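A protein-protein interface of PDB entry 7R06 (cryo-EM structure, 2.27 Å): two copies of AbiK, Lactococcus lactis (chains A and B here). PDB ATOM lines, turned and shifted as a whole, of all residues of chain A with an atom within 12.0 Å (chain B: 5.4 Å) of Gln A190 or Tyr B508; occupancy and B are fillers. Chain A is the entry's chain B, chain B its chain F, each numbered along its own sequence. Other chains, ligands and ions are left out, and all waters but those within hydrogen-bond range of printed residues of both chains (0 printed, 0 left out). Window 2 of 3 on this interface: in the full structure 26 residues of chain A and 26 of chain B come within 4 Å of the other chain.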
ATOM      1  N   HIS A 176      12.395  -9.812 -15.209  1.00  0.00           N
ATOM      2  CA  HIS A 176      11.001  -9.638 -15.604  1.00  0.00           C
ATOM      3  C   HIS A 176      10.044 -10.472 -14.770  1.00  0.00           C
ATOM      4  O   HIS A 176       8.832 -10.290 -14.890  1.00  0.00           O
ATOM      5  CB  HIS A 176      10.803  -9.955 -17.086  1.00  0.00           C
ATOM      6  CG  HIS A 176      11.391  -8.930 -18.002  1.00  0.00           C
ATOM      7  ND1 HIS A 176      10.981  -7.616 -18.017  1.00  0.00           N
ATOM      8  CD2 HIS A 176      12.352  -9.035 -18.948  1.00  0.00           C
ATOM      9  CE1 HIS A 176      11.673  -6.953 -18.926  1.00  0.00           C
ATOM     10  NE2 HIS A 176      12.508  -7.792 -19.508  1.00  0.00           N
ATOM     11  N   PRO A 179       7.874  -8.091 -11.744  1.00  0.00           N
ATOM     12  CA  PRO A 179       6.458  -7.712 -11.859  1.00  0.00           C
ATOM     13  C   PRO A 179       5.498  -8.883 -11.723  1.00  0.00           C
ATOM     14  O   PRO A 179       4.361  -8.677 -11.291  1.00  0.00           O
ATOM     15  CB  PRO A 179       6.377  -7.066 -13.250  1.00  0.00           C
ATOM     16  CG  PRO A 179       7.753  -6.638 -13.546  1.00  0.00           C
ATOM     17  CD  PRO A 179       8.629  -7.683 -12.944  1.00  0.00           C
ATOM     18  N   TRP A 180       5.907 -10.103 -12.084  1.00  0.00           N
ATOM     19  CA  TRP A 180       5.062 -11.269 -11.831  1.00  0.00           C
ATOM     20  C   TRP A 180       4.835 -11.460 -10.342  1.00  0.00           C
ATOM     21  O   TRP A 180       3.706 -11.676  -9.896  1.00  0.00           O
ATOM     22  CB  TRP A 180       5.691 -12.535 -12.404  1.00  0.00           C
ATOM     23  CG  TRP A 180       6.031 -12.503 -13.842  1.00  0.00           C
ATOM     24  CD1 TRP A 180       5.713 -11.539 -14.747  1.00  0.00           C
ATOM     25  CD2 TRP A 180       6.811 -13.471 -14.541  1.00  0.00           C
ATOM     26  NE1 TRP A 180       6.228 -11.857 -15.974  1.00  0.00           N
ATOM     27  CE2 TRP A 180       6.911 -13.040 -15.874  1.00  0.00           C
ATOM     28  CE3 TRP A 180       7.429 -14.666 -14.170  1.00  0.00           C
ATOM     29  CZ2 TRP A 180       7.601 -13.762 -16.836  1.00  0.00           C
ATOM     30  CZ3 TRP A 180       8.115 -15.379 -15.126  1.00  0.00           C
ATOM     31  CH2 TRP A 180       8.195 -14.926 -16.443  1.00  0.00           C
ATOM     32  N   ASP A 183       2.782  -8.268  -8.995  1.00  0.00           N
ATOM     33  CA  ASP A 183       1.453  -7.999  -9.527  1.00  0.00           C
ATOM     34  C   ASP A 183       0.685  -9.228  -9.994  1.00  0.00           C
ATOM     35  O   ASP A 183      -0.510  -9.111 -10.276  1.00  0.00           O
ATOM     36  CB  ASP A 183       1.542  -7.011 -10.698  1.00  0.00           C
ATOM     37  CG  ASP A 183       2.222  -5.717 -10.319  1.00  0.00           C
ATOM     38  OD1 ASP A 183       2.292  -5.414  -9.114  1.00  0.00           O
ATOM     39  OD2 ASP A 183       2.691  -5.005 -11.229  1.00  0.00           O
ATOM     40  N   GLY A 184       1.319 -10.389 -10.086  1.00  0.00           N
ATOM     41  CA  GLY A 184       0.689 -11.542 -10.697  1.00  0.00           C
ATOM     42  C   GLY A 184       1.240 -11.782 -12.085  1.00  0.00           C
ATOM     43  O   GLY A 184       1.357 -10.844 -12.877  1.00  0.00           O
ATOM     44  N   LYS A 185       1.596 -13.032 -12.389  1.00  0.00           N
ATOM     45  CA  LYS A 185       2.233 -13.324 -13.669  1.00  0.00           C
ATOM     46  C   LYS A 185       1.289 -13.084 -14.837  1.00  0.00           C
ATOM     47  O   LYS A 185       1.720 -12.610 -15.894  1.00  0.00           O
ATOM     48  CB  LYS A 185       2.748 -14.762 -13.685  1.00  0.00           C
ATOM     49  CG  LYS A 185       3.499 -15.136 -14.950  1.00  0.00           C
ATOM     50  CD  LYS A 185       3.899 -16.597 -14.931  1.00  0.00           C
ATOM     51  CE  LYS A 185       5.040 -16.871 -15.888  1.00  0.00           C
ATOM     52  NZ  LYS A 185       5.600 -18.234 -15.694  1.00  0.00           N
ATOM     53  N   SER A 186       0.002 -13.391 -14.670  1.00  0.00           N
ATOM     54  CA  SER A 186      -0.983 -13.234 -15.729  1.00  0.00           C
ATOM     55  C   SER A 186      -1.370 -11.778 -15.963  1.00  0.00           C
ATOM     56  O   SER A 186      -2.249 -11.505 -16.788  1.00  0.00           O
ATOM     57  CB  SER A 186      -2.229 -14.067 -15.421  1.00  0.00           C
ATOM     58  OG  SER A 186      -2.144 -15.343 -16.027  1.00  0.00           O
ATOM     59  N   ALA A 187      -0.741 -10.843 -15.253  1.00  0.00           N
ATOM     60  CA  ALA A 187      -0.929  -9.420 -15.496  1.00  0.00           C
ATOM     61  C   ALA A 187       0.299  -8.782 -16.132  1.00  0.00           C
ATOM     62  O   ALA A 187       0.282  -7.581 -16.425  1.00  0.00           O
ATOM     63  CB  ALA A 187      -1.289  -8.694 -14.197  1.00  0.00           C
ATOM     64  N   SER A 188       1.368  -9.554 -16.346  1.00  0.00           N
ATOM     65  CA  SER A 188       2.505  -9.058 -17.111  1.00  0.00           C
ATOM     66  C   SER A 188       2.098  -8.734 -18.540  1.00  0.00           C
ATOM     67  O   SER A 188       2.521  -7.716 -19.100  1.00  0.00           O
ATOM     68  CB  SER A 188       3.633 -10.087 -17.105  1.00  0.00           C
ATOM     69  OG  SER A 188       4.395 -10.017 -18.297  1.00  0.00           O
ATOM     70  N   LYS A 189       1.279  -9.591 -19.133  1.00  0.00           N
ATOM     71  CA  LYS A 189       0.704  -9.340 -20.443  1.00  0.00           C
ATOM     72  C   LYS A 189      -0.383  -8.281 -20.296  1.00  0.00           C
ATOM     73  O   LYS A 189      -1.296  -8.438 -19.477  1.00  0.00           O
ATOM     74  CB  LYS A 189       0.153 -10.649 -20.997  1.00  0.00           C
ATOM     75  CG  LYS A 189       1.215 -11.732 -21.022  1.00  0.00           C
ATOM     76  CD  LYS A 189       0.656 -13.103 -20.690  1.00  0.00           C
ATOM     77  CE  LYS A 189       1.523 -14.204 -21.277  1.00  0.00           C
ATOM     78  NZ  LYS A 189       1.718 -15.333 -20.327  1.00  0.00           N
ATOM     79  N   GLN A 190      -0.276  -7.204 -21.069  1.00  0.00           N
ATOM     80  CA  GLN A 190      -1.126  -6.024 -20.912  1.00  0.00           C
ATOM     81  C   GLN A 190      -2.616  -6.346 -20.838  1.00  0.00           C
ATOM     82  O   GLN A 190      -3.215  -6.291 -19.765  1.00  0.00           O
ATOM     83  CB  GLN A 190      -0.876  -5.042 -22.057  1.00  0.00           C
ATOM     84  N   LYS A 193       2.946  -1.963 -19.195  1.00  0.00           N
ATOM     85  CA  LYS A 193       3.983  -1.234 -18.473  1.00  0.00           C
ATOM     86  C   LYS A 193       3.418   0.016 -17.807  1.00  0.00           C
ATOM     87  O   LYS A 193       2.227   0.084 -17.504  1.00  0.00           O
ATOM     88  CB  LYS A 193       5.129  -0.855 -19.413  1.00  0.00           C
ATOM     89  N   LYS A 194       4.295   0.992 -17.571  1.00  0.00           N
ATOM     90  CA  LYS A 194       4.013   2.274 -16.931  1.00  0.00           C
ATOM     91  C   LYS A 194       3.675   2.134 -15.451  1.00  0.00           C
ATOM     92  O   LYS A 194       3.479   3.152 -14.780  1.00  0.00           O
ATOM     93  CB  LYS A 194       2.882   3.046 -17.630  1.00  0.00           C
ATOM     94  N   GLY A 195       3.608   0.916 -14.917  1.00  0.00           N
ATOM     95  CA  GLY A 195       3.350   0.718 -13.510  1.00  0.00           C
ATOM     96  C   GLY A 195       4.611   0.800 -12.674  1.00  0.00           C
ATOM     97  O   GLY A 195       5.718   0.996 -13.171  1.00  0.00           O
ATOM     98  N   SER A 197       6.094  -1.599 -10.677  1.00  0.00           N
ATOM     99  CA  SER A 197       7.008  -2.735 -10.723  1.00  0.00           C
ATOM    100  C   SER A 197       7.726  -2.827 -12.066  1.00  0.00           C
ATOM    101  O   SER A 197       8.903  -3.204 -12.121  1.00  0.00           O
ATOM    102  CB  SER A 197       6.248  -4.025 -10.411  1.00  0.00           C
ATOM    103  OG  SER A 197       5.354  -4.362 -11.451  1.00  0.00           O
ATOM    104  N   ASN A 198       7.042  -2.474 -13.156  1.00  0.00           N
ATOM    105  CA  ASN A 198       7.685  -2.476 -14.467  1.00  0.00           C
ATOM    106  C   ASN A 198       8.792  -1.431 -14.548  1.00  0.00           C
ATOM    107  O   ASN A 198       9.883  -1.710 -15.060  1.00  0.00           O
ATOM    108  CB  ASN A 198       6.640  -2.242 -15.557  1.00  0.00           C
ATOM    109  CG  ASN A 198       5.853  -3.496 -15.889  1.00  0.00           C
ATOM    110  OD1 ASN A 198       6.414  -4.500 -16.316  1.00  0.00           O
ATOM    111  ND2 ASN A 198       4.545  -3.440 -15.688  1.00  0.00           N
ATOM    112  N   ASP B  84       2.851 -17.209 -27.462  1.00  0.00           N
ATOM    113  CA  ASP B  84       2.993 -18.053 -26.281  1.00  0.00           C
ATOM    114  C   ASP B  84       3.112 -19.514 -26.691  1.00  0.00           C
ATOM    115  O   ASP B  84       2.345 -19.973 -27.543  1.00  0.00           O
ATOM    116  CB  ASP B  84       1.807 -17.885 -25.350  1.00  0.00           C
ATOM    117  CG  ASP B  84       2.141 -17.068 -24.135  1.00  0.00           C
ATOM    118  OD1 ASP B  84       3.057 -17.465 -23.388  1.00  0.00           O
ATOM    119  OD2 ASP B  84       1.482 -16.034 -23.919  1.00  0.00           O
ATOM    120  N   TYR B 209       7.621 -15.764 -26.215  1.00  0.00           N
ATOM    121  CA  TYR B 209       6.903 -14.553 -25.803  1.00  0.00           C
ATOM    122  C   TYR B 209       7.850 -13.488 -25.238  1.00  0.00           C
ATOM    123  O   TYR B 209       7.598 -12.900 -24.184  1.00  0.00           O
ATOM    124  CB  TYR B 209       5.795 -14.895 -24.798  1.00  0.00           C
ATOM    125  CG  TYR B 209       4.633 -13.932 -24.820  1.00  0.00           C
ATOM    126  CD1 TYR B 209       3.786 -13.868 -25.916  1.00  0.00           C
ATOM    127  CD2 TYR B 209       4.405 -13.063 -23.767  1.00  0.00           C
ATOM    128  CE1 TYR B 209       2.732 -12.985 -25.954  1.00  0.00           C
ATOM    129  CE2 TYR B 209       3.355 -12.170 -23.799  1.00  0.00           C
ATOM    130  CZ  TYR B 209       2.521 -12.133 -24.890  1.00  0.00           C
ATOM    131  OH  TYR B 209       1.475 -11.239 -24.912  1.00  0.00           O
ATOM    132  N   THR B 504      -8.704 -16.994 -20.913  1.00  0.00           N
ATOM    133  CA  THR B 504      -7.350 -16.916 -21.443  1.00  0.00           C
ATOM    134  C   THR B 504      -7.104 -15.573 -22.109  1.00  0.00           C
ATOM    135  O   THR B 504      -6.072 -14.935 -21.875  1.00  0.00           O
ATOM    136  CB  THR B 504      -7.103 -18.062 -22.417  1.00  0.00           C
ATOM    137  OG1 THR B 504      -7.659 -19.265 -21.873  1.00  0.00           O
ATOM    138  CG2 THR B 504      -5.621 -18.246 -22.632  1.00  0.00           C
ATOM    139  N   HIS B 505      -8.049 -15.120 -22.933  1.00  0.00           N
ATOM    140  CA  HIS B 505      -7.911 -13.797 -23.532  1.00  0.00           C
ATOM    141  C   HIS B 505      -7.945 -12.671 -22.509  1.00  0.00           C
ATOM    142  O   HIS B 505      -7.407 -11.593 -22.777  1.00  0.00           O
ATOM    143  CB  HIS B 505      -8.968 -13.593 -24.616  1.00  0.00           C
ATOM    144  CG  HIS B 505      -8.833 -12.292 -25.332  1.00  0.00           C
ATOM    145  ND1 HIS B 505      -8.252 -12.173 -26.574  1.00  0.00           N
ATOM    146  CD2 HIS B 505      -9.289 -11.060 -25.012  1.00  0.00           C
ATOM    147  CE1 HIS B 505      -8.285 -10.908 -26.950  1.00  0.00           C
ATOM    148  NE2 HIS B 505      -8.926 -10.216 -26.030  1.00  0.00           N
ATOM    149  N   ALA B 506      -8.524 -12.898 -21.333  1.00  0.00           N
ATOM    150  CA  ALA B 506      -8.550 -11.833 -20.337  1.00  0.00           C
ATOM    151  C   ALA B 506      -7.165 -11.499 -19.783  1.00  0.00           C
ATOM    152  O   ALA B 506      -6.985 -10.414 -19.221  1.00  0.00           O
ATOM    153  CB  ALA B 506      -9.492 -12.208 -19.192  1.00  0.00           C
ATOM    154  N   ASN B 507      -6.180 -12.380 -19.953  1.00  0.00           N
ATOM    155  CA  ASN B 507      -4.825 -12.188 -19.442  1.00  0.00           C
ATOM    156  C   ASN B 507      -3.943 -11.379 -20.383  1.00  0.00           C
ATOM    157  O   ASN B 507      -2.733 -11.296 -20.161  1.00  0.00           O
ATOM    158  CB  ASN B 507      -4.165 -13.546 -19.192  1.00  0.00           C
ATOM    159  CG  ASN B 507      -4.713 -14.244 -17.972  1.00  0.00           C
ATOM    160  OD1 ASN B 507      -4.256 -15.323 -17.606  1.00  0.00           O
ATOM    161  ND2 ASN B 507      -5.688 -13.623 -17.322  1.00  0.00           N
ATOM    162  N   TYR B 508      -4.522 -10.796 -21.422  1.00  0.00           N
ATOM    163  CA  TYR B 508      -3.842 -10.231 -22.578  1.00  0.00           C
ATOM    164  C   TYR B 508      -4.408  -8.862 -22.912  1.00  0.00           C
ATOM    165  O   TYR B 508      -5.522  -8.511 -22.523  1.00  0.00           O
ATOM    166  CB  TYR B 508      -3.993 -11.187 -23.762  1.00  0.00           C
ATOM    167  CG  TYR B 508      -3.250 -12.474 -23.566  1.00  0.00           C
ATOM    168  CD1 TYR B 508      -1.866 -12.474 -23.474  1.00  0.00           C
ATOM    169  CD2 TYR B 508      -3.890 -13.691 -23.671  1.00  0.00           C
ATOM    170  CE1 TYR B 508      -1.163 -13.645 -23.362  1.00  0.00           C
ATOM    171  CE2 TYR B 508      -3.198 -14.869 -23.521  1.00  0.00           C
ATOM    172  CZ  TYR B 508      -1.829 -14.840 -23.388  1.00  0.00           C
ATOM    173  OH  TYR B 508      -1.127 -16.011 -23.266  1.00  0.00           O
ATOM    174  N   ASP B 509      -3.618  -8.081 -23.640  1.00  0.00           N
ATOM    175  CA  ASP B 509      -4.122  -6.831 -24.181  1.00  0.00           C
ATOM    176  C   ASP B 509      -5.257  -7.138 -25.150  1.00  0.00           C
ATOM    177  O   ASP B 509      -5.228  -8.132 -25.877  1.00  0.00           O
ATOM    178  CB  ASP B 509      -2.983  -6.058 -24.864  1.00  0.00           C
ATOM    179  CG  ASP B 509      -3.438  -4.755 -25.523  1.00  0.00           C
ATOM    180  OD1 ASP B 509      -4.634  -4.572 -25.822  1.00  0.00           O
ATOM    181  OD2 ASP B 509      -2.573  -3.888 -25.740  1.00  0.00           O
ATOM    182  N   VAL B 510      -6.273  -6.274 -25.150  1.00  0.00           N
ATOM    183  CA  VAL B 510      -7.466  -6.529 -25.948  1.00  0.00           C
ATOM    184  C   VAL B 510      -7.197  -6.484 -27.442  1.00  0.00           C
ATOM    185  O   VAL B 510      -8.043  -6.926 -28.227  1.00  0.00           O
ATOM    186  CB  VAL B 510      -8.585  -5.532 -25.585  1.00  0.00           C
ATOM    187  CG1 VAL B 510      -9.041  -5.754 -24.155  1.00  0.00           C
ATOM    188  CG2 VAL B 510      -8.107  -4.108 -25.773  1.00  0.00           C
ATOM    189  N   THR B 512      -4.546  -8.105 -28.650  1.00  0.00           N
ATOM    190  CA  THR B 512      -3.733  -9.284 -28.907  1.00  0.00           C
ATOM    191  C   THR B 512      -4.557 -10.325 -29.653  1.00  0.00           C
ATOM    192  O   THR B 512      -5.672 -10.658 -29.243  1.00  0.00           O
ATOM    193  CB  THR B 512      -3.204  -9.867 -27.599  1.00  0.00           C
ATOM    194  OG1 THR B 512      -2.247  -8.970 -27.028  1.00  0.00           O
ATOM    195  CG2 THR B 512      -2.531 -11.198 -27.846  1.00  0.00           C
ATOM    196  N   GLU B 517      -1.717 -16.299 -28.597  1.00  0.00           N
ATOM    197  CA  GLU B 517      -1.907 -16.400 -27.161  1.00  0.00           C
ATOM    198  C   GLU B 517      -1.681 -17.833 -26.689  1.00  0.00           C
ATOM    199  O   GLU B 517      -1.402 -18.742 -27.470  1.00  0.00           O
ATOM    200  CB  GLU B 517      -3.311 -15.942 -26.780  1.00  0.00           C
ATOM    201  CG  GLU B 517      -3.511 -14.456 -26.825  1.00  0.00           C
ATOM    202  CD  GLU B 517      -4.977 -14.070 -26.836  1.00  0.00           C
ATOM    203  OE1 GLU B 517      -5.278 -12.866 -26.735  1.00  0.00           O
ATOM    204  OE2 GLU B 517      -5.830 -14.975 -26.919  1.00  0.00           O
ATOM    205  N   LYS B 518      -1.819 -18.031 -25.382  1.00  0.00           N
ATOM    206  CA  LYS B 518      -1.852 -19.378 -24.833  1.00  0.00           C
ATOM    207  C   LYS B 518      -3.056 -20.140 -25.371  1.00  0.00           C
ATOM    208  O   LYS B 518      -4.088 -19.558 -25.707  1.00  0.00           O
ATOM    209  CB  LYS B 518      -1.902 -19.342 -23.307  1.00  0.00           C
ATOM    210  CG  LYS B 518      -0.600 -19.715 -22.642  1.00  0.00           C
ATOM    211  CD  LYS B 518      -0.775 -19.912 -21.148  1.00  0.00           C
ATOM    212  CE  LYS B 518       0.548 -19.750 -20.415  1.00  0.00           C
ATOM    213  NZ  LYS B 518       0.750 -20.818 -19.397  1.00  0.00           N
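Of the printed residues of chain B, Ser A186 touches Asn B507.
Ser A188 touches none of the printed residues of chain B.
Gln A190 touches just these residues of chain B: Tyr B508 and Asp B509.
Gly A195 touches none of the printed residues of chain B.
Of chain A, only Lys A189 (3.2 Å) comes within 4 Å of Asp B84.
Printed residues of chain A within 4 Å of Tyr B209: Lys A189 (3.5 Å).
No residue of chain A comes within 4 Å of Thr B504.
No residue of chain A comes within 4 Å of His B505.
No residue of chain A comes within 4 Å of Ala B506.
Printed residues of chain A within 4 Å of Asn B507: Ser A186 (2.6 Å) and Lys A189 (3.1 Å).
Of chain A, only Lys A189 and Gln A190 come within 4 Å of Tyr B508.
No residue of chain A comes within 4 Å of Val B510.
No residue of chain A comes within 4 Å of Glu B517.
No residue of chain A comes within 4 Å of Lys B518.
The side-chain carboxylate (OD2) of Asp B84 sits at hydrogen-bond distance from the side-chain hydroxyl (OH) of Tyr B508.
The side-chain hydroxyl (OH) of Tyr B508 sits at hydrogen-bond distance from the backbone NH (N) of Lys B518 (3.0 Å).
The side-chain hydroxyl (OG1) of Thr B512 sits close to the backbone carbonyl oxygen (O) of Asp B509 (3.3 Å).
No position is printed for both chains.
The side-chain amide oxygen (OD1) of Asn B507 is in hydrogen-bond range of the side-chain hydroxyl (OG) of Ser A186 (2.6 Å).
The side-chain amino group (NZ) of Lys A189 lies within salt-bridge range of the side-chain carboxylate (OD2) of Asp B84.
The backbone carbonyl oxygen (O) of Lys A189 sits close to the backbone carbonyl oxygen (O) of Asn B507 (3.3 Å).
Hydrophobic or aromatic side chains of chain B within 4 Å of the printed part of chain A: Tyr B209 and Tyr B508.
Among the printed residues, Asp or Glu carboxylates within 4 Å of a Lys or Arg side-chain nitrogen of the other chain: Lys A189 with Asp B84 (3.7 Å).
Lys A189 touches Tyr B209 (CG to CE2, 3.5 Å).
CD of Lys A189 touches CE1 of Tyr B508 (3.3 Å).
Gln A190 touches Tyr B508.
C of Gln A190 touches N of Asp B509, 3.4 Å away.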
